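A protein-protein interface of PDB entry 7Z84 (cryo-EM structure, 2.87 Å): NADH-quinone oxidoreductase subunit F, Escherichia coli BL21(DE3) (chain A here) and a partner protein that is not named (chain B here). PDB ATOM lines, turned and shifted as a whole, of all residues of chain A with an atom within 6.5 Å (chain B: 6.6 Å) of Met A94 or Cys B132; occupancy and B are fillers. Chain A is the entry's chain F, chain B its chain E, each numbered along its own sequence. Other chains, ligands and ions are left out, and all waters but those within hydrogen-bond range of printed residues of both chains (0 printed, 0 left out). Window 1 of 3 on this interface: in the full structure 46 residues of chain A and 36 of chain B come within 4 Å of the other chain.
The side-chain sulfur (SG) of Cys B133 lies close to the backbone carbonyl oxygen (O) of Glu A95, at 3.8 Å. The guanidinium group (NH2) of Arg A133 sits at hydrogen-bond distance from the backbone carbonyl oxygen (O) of Cys B133 (2.6 Å). The backbone carbonyl oxygen of Thr B131 sits close to the guanidinium group of Arg A348 (3.3 Å). The backbone carbonyl oxygen of Ala A175 lies close to the backbone NH of Gln B78 (3.2 Å). O of Gly A176 sits close to OG of Ser B77 (2.4 Å). The side-chain sulfur (SD) of Met A94 lies within hydrogen-bond range of the side-chain sulfur (SG) of Cys B132 (3.6 Å). The side-chain carboxylate (OD2) of Asp B93 lies within salt-bridge range of the guanidinium group (NH1) of Arg A348 (2.6 Å).
NE2 of Gln B78 lies within hydrogen-bond range of OG of Ser B77, 3.1 Å away. The backbone carbonyl oxygen of Ala A91 sits at hydrogen-bond distance from the backbone NH of Arg A133. OG1 of Thr A98 lies close to O of Glu A95, 3.3 Å away. N of Asp B93 is in hydrogen-bond range of O of Thr B131 (3.1 Å). The side-chain sulfur (SD) of Met A94 lies within hydrogen-bond range of the guanidinium group (NH2) of Arg A133 (3.7 Å). The backbone carbonyl oxygen (O) of Glu A93 lies within hydrogen-bond range of the guanidinium group (NH1) of Arg A133, 3.4 Å away.
Of chain B, only Cys B132 (3.6 Å) comes within 4 Å of Met A94. Of chain A, only Met A94 (3.6 Å), Phe A345 (3.7 Å) and Arg A348 (3.5 Å) come within 4 Å of Cys B132. Of the printed residues of chain A, Ser B77 touches Ala A175 (3.8 Å), Gly A176 (2.4 Å) and Arg A177 (3.8 Å). Printed residues of chain B within 4 Å of Glu A135: Gln B78 (3.5 Å) and Leu B134 (3.8 Å). Printed residues of chain B within 4 Å of Arg A348: Asp B93 (2.4 Å), Thr B131 (3.3 Å) and Cys B132 (3.5 Å). Cys B92 touches none of the printed residues of chain A. The nearest residue of chain A that does not touch Cys B132 is Glu A349 (4.3 Å).
Among the printed residues, merely in contact across the chains: Tyr A136 with Gly B135 (3.3 Å), Tyr A136 with Leu B134 (3.4 Å), Arg A348 with Cys B132 (3.5 Å), Glu A135 with Gln B78 (3.5 Å), Pro A96 with Cys B133 (3.6 Å), Thr A98 with Gly B135 (3.6 Å), Phe A345 with Cys B132 (3.7 Å), Arg A133 with Leu B134 (3.7 Å), Gly A176 with Gln B78 (3.7 Å), Arg A133 with Gly B135 (3.7 Å), Ala A175 with Ser B77 (3.8 Å), Glu A135 with Leu B134 (3.8 Å), Arg A177 with Ser B77 (3.8 Å) and Pro A96 with Ser B94 (3.9 Å).
Of the 20 printed residues of chain A, 12 touch a printed residue of chain B. Along chain B the printed residues that touch a printed residue of chain A span positions 77 to 135. Among the printed residues, 21 pairs touch across the chains. Among the printed residues, Asp or Glu carboxylates within 4 Å of a Lys or Arg side-chain nitrogen of the other chain: Arg A348 with Asp B93 (2.4 Å).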
ATOM      1  N   ALA A  91     -23.881  13.260  -8.606  1.00  0.00           N
ATOM      2  CA  ALA A  91     -22.438  13.312  -8.466  1.00  0.00           C
ATOM      3  C   ALA A  91     -21.861  12.001  -7.951  1.00  0.00           C
ATOM      4  O   ALA A  91     -20.775  12.002  -7.361  1.00  0.00           O
ATOM      5  CB  ALA A  91     -22.050  14.463  -7.537  1.00  0.00           C
ATOM      6  N   ASP A  92     -22.574  10.890  -8.148  1.00  0.00           N
ATOM      7  CA  ASP A  92     -22.072   9.591  -7.715  1.00  0.00           C
ATOM      8  C   ASP A  92     -20.858   9.176  -8.537  1.00  0.00           C
ATOM      9  O   ASP A  92     -19.752   9.060  -8.002  1.00  0.00           O
ATOM     10  CB  ASP A  92     -23.180   8.543  -7.814  1.00  0.00           C
ATOM     11  CG  ASP A  92     -23.030   7.436  -6.790  1.00  0.00           C
ATOM     12  OD1 ASP A  92     -22.296   7.636  -5.799  1.00  0.00           O
ATOM     13  OD2 ASP A  92     -23.642   6.365  -6.974  1.00  0.00           O
ATOM     14  N   GLU A  93     -21.048   8.989  -9.848  1.00  0.00           N
ATOM     15  CA  GLU A  93     -19.981   8.650 -10.799  1.00  0.00           C
ATOM     16  C   GLU A  93     -19.209   7.405 -10.363  1.00  0.00           C
ATOM     17  O   GLU A  93     -17.986   7.416 -10.215  1.00  0.00           O
ATOM     18  CB  GLU A  93     -19.034   9.831 -11.012  1.00  0.00           C
ATOM     19  CG  GLU A  93     -18.374   9.845 -12.375  1.00  0.00           C
ATOM     20  CD  GLU A  93     -17.050  10.572 -12.371  1.00  0.00           C
ATOM     21  OE1 GLU A  93     -16.418  10.655 -11.298  1.00  0.00           O
ATOM     22  OE2 GLU A  93     -16.645  11.067 -13.441  1.00  0.00           O
ATOM     23  N   MET A  94     -19.944   6.321 -10.144  1.00  0.00           N
ATOM     24  CA  MET A  94     -19.368   5.093  -9.622  1.00  0.00           C
ATOM     25  C   MET A  94     -19.000   4.097 -10.712  1.00  0.00           C
ATOM     26  O   MET A  94     -18.563   2.988 -10.394  1.00  0.00           O
ATOM     27  CB  MET A  94     -20.337   4.449  -8.628  1.00  0.00           C
ATOM     28  CG  MET A  94     -20.091   4.830  -7.185  1.00  0.00           C
ATOM     29  SD  MET A  94     -19.119   3.593  -6.317  1.00  0.00           S
ATOM     30  CE  MET A  94     -19.453   4.037  -4.620  1.00  0.00           C
ATOM     31  N   GLU A  95     -19.164   4.461 -11.978  1.00  0.00           N
ATOM     32  CA  GLU A  95     -18.813   3.559 -13.069  1.00  0.00           C
ATOM     33  C   GLU A  95     -17.298   3.438 -13.186  1.00  0.00           C
ATOM     34  O   GLU A  95     -16.599   4.458 -13.171  1.00  0.00           O
ATOM     35  CB  GLU A  95     -19.390   4.060 -14.387  1.00  0.00           C
ATOM     36  CG  GLU A  95     -19.045   3.202 -15.589  1.00  0.00           C
ATOM     37  CD  GLU A  95     -20.116   2.177 -15.898  1.00  0.00           C
ATOM     38  OE1 GLU A  95     -20.348   1.286 -15.058  1.00  0.00           O
ATOM     39  OE2 GLU A  95     -20.727   2.262 -16.984  1.00  0.00           O
ATOM     40  N   PRO A  96     -16.758   2.224 -13.275  1.00  0.00           N
ATOM     41  CA  PRO A  96     -15.326   2.073 -13.552  1.00  0.00           C
ATOM     42  C   PRO A  96     -14.965   2.621 -14.923  1.00  0.00           C
ATOM     43  O   PRO A  96     -15.673   2.404 -15.908  1.00  0.00           O
ATOM     44  CB  PRO A  96     -15.106   0.559 -13.469  1.00  0.00           C
ATOM     45  CG  PRO A  96     -16.227   0.063 -12.616  1.00  0.00           C
ATOM     46  CD  PRO A  96     -17.393   0.943 -12.935  1.00  0.00           C
ATOM     47  N   THR A  98     -14.733   5.922 -15.325  1.00  0.00           N
ATOM     48  CA  THR A  98     -15.299   7.264 -15.356  1.00  0.00           C
ATOM     49  C   THR A  98     -14.661   8.104 -14.259  1.00  0.00           C
ATOM     50  O   THR A  98     -14.721   7.744 -13.079  1.00  0.00           O
ATOM     51  CB  THR A  98     -16.817   7.226 -15.190  1.00  0.00           C
ATOM     52  OG1 THR A  98     -17.347   6.117 -15.922  1.00  0.00           O
ATOM     53  CG2 THR A  98     -17.434   8.507 -15.718  1.00  0.00           C
ATOM     54  N   ARG A 133     -20.759  10.880  -4.061  1.00  0.00           N
ATOM     55  CA  ARG A 133     -20.189   9.665  -3.499  1.00  0.00           C
ATOM     56  C   ARG A 133     -19.287  10.016  -2.320  1.00  0.00           C
ATOM     57  O   ARG A 133     -18.745  11.120  -2.229  1.00  0.00           O
ATOM     58  CB  ARG A 133     -19.410   8.887  -4.563  1.00  0.00           C
ATOM     59  CG  ARG A 133     -18.076   9.495  -4.956  1.00  0.00           C
ATOM     60  CD  ARG A 133     -17.352   8.638  -5.984  1.00  0.00           C
ATOM     61  NE  ARG A 133     -16.890   7.358  -5.462  1.00  0.00           N
ATOM     62  CZ  ARG A 133     -16.328   6.414  -6.202  1.00  0.00           C
ATOM     63  NH1 ARG A 133     -16.161   6.566  -7.504  1.00  0.00           N
ATOM     64  NH2 ARG A 133     -15.919   5.291  -5.620  1.00  0.00           N
ATOM     65  N   GLY A 134     -19.143   9.065  -1.399  1.00  0.00           N
ATOM     66  CA  GLY A 134     -18.359   9.312  -0.203  1.00  0.00           C
ATOM     67  C   GLY A 134     -16.861   9.309  -0.420  1.00  0.00           C
ATOM     68  O   GLY A 134     -16.120   9.671   0.498  1.00  0.00           O
ATOM     69  N   GLU A 135     -16.407   8.913  -1.605  1.00  0.00           N
ATOM     70  CA  GLU A 135     -14.989   8.831  -1.918  1.00  0.00           C
ATOM     71  C   GLU A 135     -14.430  10.124  -2.495  1.00  0.00           C
ATOM     72  O   GLU A 135     -13.211  10.232  -2.664  1.00  0.00           O
ATOM     73  CB  GLU A 135     -14.734   7.679  -2.896  1.00  0.00           C
ATOM     74  CG  GLU A 135     -14.964   6.283  -2.318  1.00  0.00           C
ATOM     75  CD  GLU A 135     -16.431   5.890  -2.247  1.00  0.00           C
ATOM     76  OE1 GLU A 135     -17.162   6.120  -3.231  1.00  0.00           O
ATOM     77  OE2 GLU A 135     -16.854   5.353  -1.201  1.00  0.00           O
ATOM     78  N   TYR A 136     -15.284  11.101  -2.803  1.00  0.00           N
ATOM     79  CA  TYR A 136     -14.846  12.388  -3.338  1.00  0.00           C
ATOM     80  C   TYR A 136     -14.821  13.390  -2.188  1.00  0.00           C
ATOM     81  O   TYR A 136     -15.711  14.224  -2.026  1.00  0.00           O
ATOM     82  CB  TYR A 136     -15.759  12.846  -4.473  1.00  0.00           C
ATOM     83  CG  TYR A 136     -15.601  12.089  -5.776  1.00  0.00           C
ATOM     84  CD1 TYR A 136     -14.621  11.116  -5.934  1.00  0.00           C
ATOM     85  CD2 TYR A 136     -16.437  12.354  -6.853  1.00  0.00           C
ATOM     86  CE1 TYR A 136     -14.481  10.428  -7.125  1.00  0.00           C
ATOM     87  CE2 TYR A 136     -16.305  11.672  -8.047  1.00  0.00           C
ATOM     88  CZ  TYR A 136     -15.327  10.711  -8.176  1.00  0.00           C
ATOM     89  OH  TYR A 136     -15.194  10.031  -9.364  1.00  0.00           O
ATOM     90  N   ALA A 175     -22.755   6.816   0.921  1.00  0.00           N
ATOM     91  CA  ALA A 175     -22.145   5.792   1.757  1.00  0.00           C
ATOM     92  C   ALA A 175     -21.612   4.622   0.935  1.00  0.00           C
ATOM     93  O   ALA A 175     -21.632   3.478   1.390  1.00  0.00           O
ATOM     94  CB  ALA A 175     -23.136   5.296   2.809  1.00  0.00           C
ATOM     95  N   GLY A 176     -21.152   4.891  -0.284  1.00  0.00           N
ATOM     96  CA  GLY A 176     -20.375   3.919  -1.028  1.00  0.00           C
ATOM     97  C   GLY A 176     -21.115   2.723  -1.591  1.00  0.00           C
ATOM     98  O   GLY A 176     -20.884   1.592  -1.158  1.00  0.00           O
ATOM     99  N   ARG A 177     -22.004   2.952  -2.555  1.00  0.00           N
ATOM    100  CA  ARG A 177     -22.660   1.856  -3.253  1.00  0.00           C
ATOM    101  C   ARG A 177     -22.914   2.282  -4.693  1.00  0.00           C
ATOM    102  O   ARG A 177     -23.372   3.400  -4.942  1.00  0.00           O
ATOM    103  CB  ARG A 177     -23.963   1.453  -2.553  1.00  0.00           C
ATOM    104  CG  ARG A 177     -24.585   0.168  -3.067  1.00  0.00           C
ATOM    105  CD  ARG A 177     -23.596  -0.984  -3.037  1.00  0.00           C
ATOM    106  NE  ARG A 177     -23.569  -1.681  -1.759  1.00  0.00           N
ATOM    107  CZ  ARG A 177     -22.848  -2.768  -1.518  1.00  0.00           C
ATOM    108  NH1 ARG A 177     -22.079  -3.308  -2.447  1.00  0.00           N
ATOM    109  NH2 ARG A 177     -22.904  -3.331  -0.313  1.00  0.00           N
ATOM    110  N   TYR A 178     -22.609   1.383  -5.632  1.00  0.00           N
ATOM    111  CA  TYR A 178     -22.633   1.731  -7.052  1.00  0.00           C
ATOM    112  C   TYR A 178     -24.049   1.946  -7.569  1.00  0.00           C
ATOM    113  O   TYR A 178     -24.262   2.792  -8.443  1.00  0.00           O
ATOM    114  CB  TYR A 178     -21.926   0.641  -7.861  1.00  0.00           C
ATOM    115  CG  TYR A 178     -22.208   0.647  -9.350  1.00  0.00           C
ATOM    116  CD1 TYR A 178     -21.579   1.552 -10.192  1.00  0.00           C
ATOM    117  CD2 TYR A 178     -23.079  -0.273  -9.915  1.00  0.00           C
ATOM    118  CE1 TYR A 178     -21.824   1.555 -11.548  1.00  0.00           C
ATOM    119  CE2 TYR A 178     -23.329  -0.275 -11.272  1.00  0.00           C
ATOM    120  CZ  TYR A 178     -22.699   0.638 -12.082  1.00  0.00           C
ATOM    121  OH  TYR A 178     -22.945   0.634 -13.433  1.00  0.00           O
ATOM    122  N   ILE A 179     -25.024   1.199  -7.043  1.00  0.00           N
ATOM    123  CA  ILE A 179     -26.399   1.285  -7.525  1.00  0.00           C
ATOM    124  C   ILE A 179     -27.054   2.618  -7.183  1.00  0.00           C
ATOM    125  O   ILE A 179     -28.060   2.981  -7.802  1.00  0.00           O
ATOM    126  CB  ILE A 179     -27.203   0.089  -6.966  1.00  0.00           C
ATOM    127  CG1 ILE A 179     -28.508  -0.140  -7.742  1.00  0.00           C
ATOM    128  CG2 ILE A 179     -27.489   0.273  -5.487  1.00  0.00           C
ATOM    129  CD1 ILE A 179     -28.375  -0.017  -9.247  1.00  0.00           C
ATOM    130  N   GLY A 181     -26.171   5.452  -8.070  1.00  0.00           N
ATOM    131  CA  GLY A 181     -26.172   6.344  -9.212  1.00  0.00           C
ATOM    132  C   GLY A 181     -27.409   6.253 -10.076  1.00  0.00           C
ATOM    133  O   GLY A 181     -27.705   7.201 -10.810  1.00  0.00           O
ATOM    134  N   PHE A 345     -17.256  -7.118 -10.268  1.00  0.00           N
ATOM    135  CA  PHE A 345     -17.747  -5.802  -9.870  1.00  0.00           C
ATOM    136  C   PHE A 345     -19.261  -5.722  -9.996  1.00  0.00           C
ATOM    137  O   PHE A 345     -19.950  -5.295  -9.063  1.00  0.00           O
ATOM    138  CB  PHE A 345     -17.092  -4.705 -10.714  1.00  0.00           C
ATOM    139  CG  PHE A 345     -17.801  -3.379 -10.632  1.00  0.00           C
ATOM    140  CD1 PHE A 345     -17.627  -2.557  -9.532  1.00  0.00           C
ATOM    141  CD2 PHE A 345     -18.647  -2.956 -11.650  1.00  0.00           C
ATOM    142  CE1 PHE A 345     -18.275  -1.342  -9.449  1.00  0.00           C
ATOM    143  CE2 PHE A 345     -19.306  -1.749 -11.564  1.00  0.00           C
ATOM    144  CZ  PHE A 345     -19.119  -0.941 -10.463  1.00  0.00           C
ATOM    145  N   ARG A 348     -21.065  -7.961  -7.370  1.00  0.00           N
ATOM    146  CA  ARG A 348     -21.022  -7.505  -5.987  1.00  0.00           C
ATOM    147  C   ARG A 348     -21.629  -6.120  -5.799  1.00  0.00           C
ATOM    148  O   ARG A 348     -21.761  -5.672  -4.657  1.00  0.00           O
ATOM    149  CB  ARG A 348     -19.585  -7.514  -5.459  1.00  0.00           C
ATOM    150  CG  ARG A 348     -18.773  -6.287  -5.808  1.00  0.00           C
ATOM    151  CD  ARG A 348     -17.348  -6.426  -5.320  1.00  0.00           C
ATOM    152  NE  ARG A 348     -16.571  -5.227  -5.597  1.00  0.00           N
ATOM    153  CZ  ARG A 348     -15.261  -5.125  -5.424  1.00  0.00           C
ATOM    154  NH1 ARG A 348     -14.543  -6.141  -4.974  1.00  0.00           N
ATOM    155  NH2 ARG A 348     -14.659  -3.974  -5.703  1.00  0.00           N
ATOM    156  N   GLU A 349     -21.993  -5.429  -6.876  1.00  0.00           N
ATOM    157  CA  GLU A 349     -22.662  -4.140  -6.774  1.00  0.00           C
ATOM    158  C   GLU A 349     -24.138  -4.222  -7.128  1.00  0.00           C
ATOM    159  O   GLU A 349     -24.782  -3.184  -7.311  1.00  0.00           O
ATOM    160  CB  GLU A 349     -21.963  -3.099  -7.648  1.00  0.00           C
ATOM    161  CG  GLU A 349     -20.561  -2.751  -7.177  1.00  0.00           C
ATOM    162  CD  GLU A 349     -20.518  -2.242  -5.751  1.00  0.00           C
ATOM    163  OE1 GLU A 349     -21.387  -1.430  -5.379  1.00  0.00           O
ATOM    164  OE2 GLU A 349     -19.609  -2.653  -5.001  1.00  0.00           O
ATOM    165  N   SER B  77     -21.724  -0.305   1.698  1.00  0.00           N
ATOM    166  CA  SER B  77     -20.437  -0.932   1.975  1.00  0.00           C
ATOM    167  C   SER B  77     -19.548  -0.057   2.849  1.00  0.00           C
ATOM    168  O   SER B  77     -18.705  -0.580   3.585  1.00  0.00           O
ATOM    169  CB  SER B  77     -19.728  -1.265   0.663  1.00  0.00           C
ATOM    170  OG  SER B  77     -19.592  -0.113  -0.147  1.00  0.00           O
ATOM    171  N   GLN B  78     -19.715   1.262   2.793  1.00  0.00           N
ATOM    172  CA  GLN B  78     -18.870   2.168   3.557  1.00  0.00           C
ATOM    173  C   GLN B  78     -19.367   2.392   4.978  1.00  0.00           C
ATOM    174  O   GLN B  78     -18.718   3.118   5.736  1.00  0.00           O
ATOM    175  CB  GLN B  78     -18.741   3.515   2.840  1.00  0.00           C
ATOM    176  CG  GLN B  78     -17.819   3.516   1.624  1.00  0.00           C
ATOM    177  CD  GLN B  78     -16.813   2.379   1.621  1.00  0.00           C
ATOM    178  OE1 GLN B  78     -15.848   2.382   2.386  1.00  0.00           O
ATOM    179  NE2 GLN B  78     -17.035   1.399   0.753  1.00  0.00           N
ATOM    180  N   TYR B  91      -8.249  -0.621  -1.421  1.00  0.00           N
ATOM    181  CA  TYR B  91      -7.575  -0.663  -2.712  1.00  0.00           C
ATOM    182  C   TYR B  91      -8.586  -0.925  -3.818  1.00  0.00           C
ATOM    183  O   TYR B  91      -9.500  -1.738  -3.661  1.00  0.00           O
ATOM    184  CB  TYR B  91      -6.461  -1.718  -2.732  1.00  0.00           C
ATOM    185  CG  TYR B  91      -6.918  -3.156  -2.625  1.00  0.00           C
ATOM    186  CD1 TYR B  91      -7.103  -3.754  -1.387  1.00  0.00           C
ATOM    187  CD2 TYR B  91      -7.129  -3.926  -3.762  1.00  0.00           C
ATOM    188  CE1 TYR B  91      -7.512  -5.070  -1.285  1.00  0.00           C
ATOM    189  CE2 TYR B  91      -7.540  -5.237  -3.670  1.00  0.00           C
ATOM    190  CZ  TYR B  91      -7.728  -5.805  -2.430  1.00  0.00           C
ATOM    191  OH  TYR B  91      -8.133  -7.116  -2.336  1.00  0.00           O
ATOM    192  N   CYS B  92      -8.426  -0.213  -4.929  1.00  0.00           N
ATOM    193  CA  CYS B  92      -9.338  -0.362  -6.055  1.00  0.00           C
ATOM    194  C   CYS B  92      -9.050  -1.660  -6.799  1.00  0.00           C
ATOM    195  O   CYS B  92      -7.890  -1.991  -7.061  1.00  0.00           O
ATOM    196  CB  CYS B  92      -9.205   0.834  -6.994  1.00  0.00           C
ATOM    197  SG  CYS B  92     -10.259   0.759  -8.445  1.00  0.00           S
ATOM    198  N   ASP B  93     -10.108  -2.402  -7.138  1.00  0.00           N
ATOM    199  CA  ASP B  93      -9.959  -3.654  -7.870  1.00  0.00           C
ATOM    200  C   ASP B  93     -10.821  -3.674  -9.128  1.00  0.00           C
ATOM    201  O   ASP B  93     -11.190  -4.745  -9.614  1.00  0.00           O
ATOM    202  CB  ASP B  93     -10.271  -4.859  -6.977  1.00  0.00           C
ATOM    203  CG  ASP B  93     -11.712  -4.902  -6.493  1.00  0.00           C
ATOM    204  OD1 ASP B  93     -12.456  -3.915  -6.653  1.00  0.00           O
ATOM    205  OD2 ASP B  93     -12.107  -5.946  -5.938  1.00  0.00           O
ATOM    206  N   SER B  94     -11.146  -2.505  -9.667  1.00  0.00           N
ATOM    207  CA  SER B  94     -12.014  -2.425 -10.830  1.00  0.00           C
ATOM    208  C   SER B  94     -11.190  -2.622 -12.102  1.00  0.00           C
ATOM    209  O   SER B  94     -10.007  -2.968 -12.056  1.00  0.00           O
ATOM    210  CB  SER B  94     -12.782  -1.108 -10.828  1.00  0.00           C
ATOM    211  OG  SER B  94     -13.773  -1.100  -9.817  1.00  0.00           O
ATOM    212  N   PRO B 130     -10.906  -4.485  -0.293  1.00  0.00           N
ATOM    213  CA  PRO B 130     -11.112  -4.089  -1.685  1.00  0.00           C
ATOM    214  C   PRO B 130     -12.257  -3.098  -1.783  1.00  0.00           C
ATOM    215  O   PRO B 130     -13.160  -3.067  -0.944  1.00  0.00           O
ATOM    216  CB  PRO B 130     -11.454  -5.408  -2.384  1.00  0.00           C
ATOM    217  CG  PRO B 130     -12.067  -6.239  -1.313  1.00  0.00           C
ATOM    218  CD  PRO B 130     -11.389  -5.851  -0.025  1.00  0.00           C
ATOM    219  N   THR B 131     -12.207  -2.273  -2.822  1.00  0.00           N
ATOM    220  CA  THR B 131     -13.264  -1.307  -3.065  1.00  0.00           C
ATOM    221  C   THR B 131     -13.400  -1.118  -4.565  1.00  0.00           C
ATOM    222  O   THR B 131     -12.500  -1.453  -5.337  1.00  0.00           O
ATOM    223  CB  THR B 131     -12.990   0.032  -2.362  1.00  0.00           C
ATOM    224  OG1 THR B 131     -14.185   0.822  -2.351  1.00  0.00           O
ATOM    225  CG2 THR B 131     -11.885   0.804  -3.064  1.00  0.00           C
ATOM    226  N   CYS B 132     -14.529  -0.552  -4.969  1.00  0.00           N
ATOM    227  CA  CYS B 132     -14.821  -0.354  -6.381  1.00  0.00           C
ATOM    228  C   CYS B 132     -14.003   0.826  -6.905  1.00  0.00           C
ATOM    229  O   CYS B 132     -13.087   1.329  -6.247  1.00  0.00           O
ATOM    230  CB  CYS B 132     -16.319  -0.163  -6.588  1.00  0.00           C
ATOM    231  SG  CYS B 132     -17.123   0.815  -5.305  1.00  0.00           S
ATOM    232  N   CYS B 133     -14.317   1.258  -8.125  1.00  0.00           N
ATOM    233  CA  CYS B 133     -13.551   2.311  -8.778  1.00  0.00           C
ATOM    234  C   CYS B 133     -13.649   3.622  -8.010  1.00  0.00           C
ATOM    235  O   CYS B 133     -14.741   4.065  -7.643  1.00  0.00           O
ATOM    236  CB  CYS B 133     -14.045   2.503 -10.205  1.00  0.00           C
ATOM    237  SG  CYS B 133     -13.559   4.062 -10.951  1.00  0.00           S
ATOM    238  N   LEU B 134     -12.497   4.237  -7.770  1.00  0.00           N
ATOM    239  CA  LEU B 134     -12.402   5.449  -6.974  1.00  0.00           C
ATOM    240  C   LEU B 134     -12.509   6.711  -7.815  1.00  0.00           C
ATOM    241  O   LEU B 134     -12.333   7.811  -7.284  1.00  0.00           O
ATOM    242  CB  LEU B 134     -11.089   5.453  -6.190  1.00  0.00           C
ATOM    243  CG  LEU B 134     -10.966   4.374  -5.115  1.00  0.00           C
ATOM    244  CD1 LEU B 134      -9.558   4.337  -4.550  1.00  0.00           C
ATOM    245  CD2 LEU B 134     -11.980   4.610  -4.012  1.00  0.00           C
ATOM    246  N   GLY B 135     -12.799   6.579  -9.106  1.00  0.00           N
ATOM    247  CA  GLY B 135     -12.850   7.733  -9.979  1.00  0.00           C
ATOM    248  C   GLY B 135     -11.501   8.350 -10.257  1.00  0.00           C
ATOM    249  O   GLY B 135     -11.415   9.556 -10.492  1.00  0.00           O
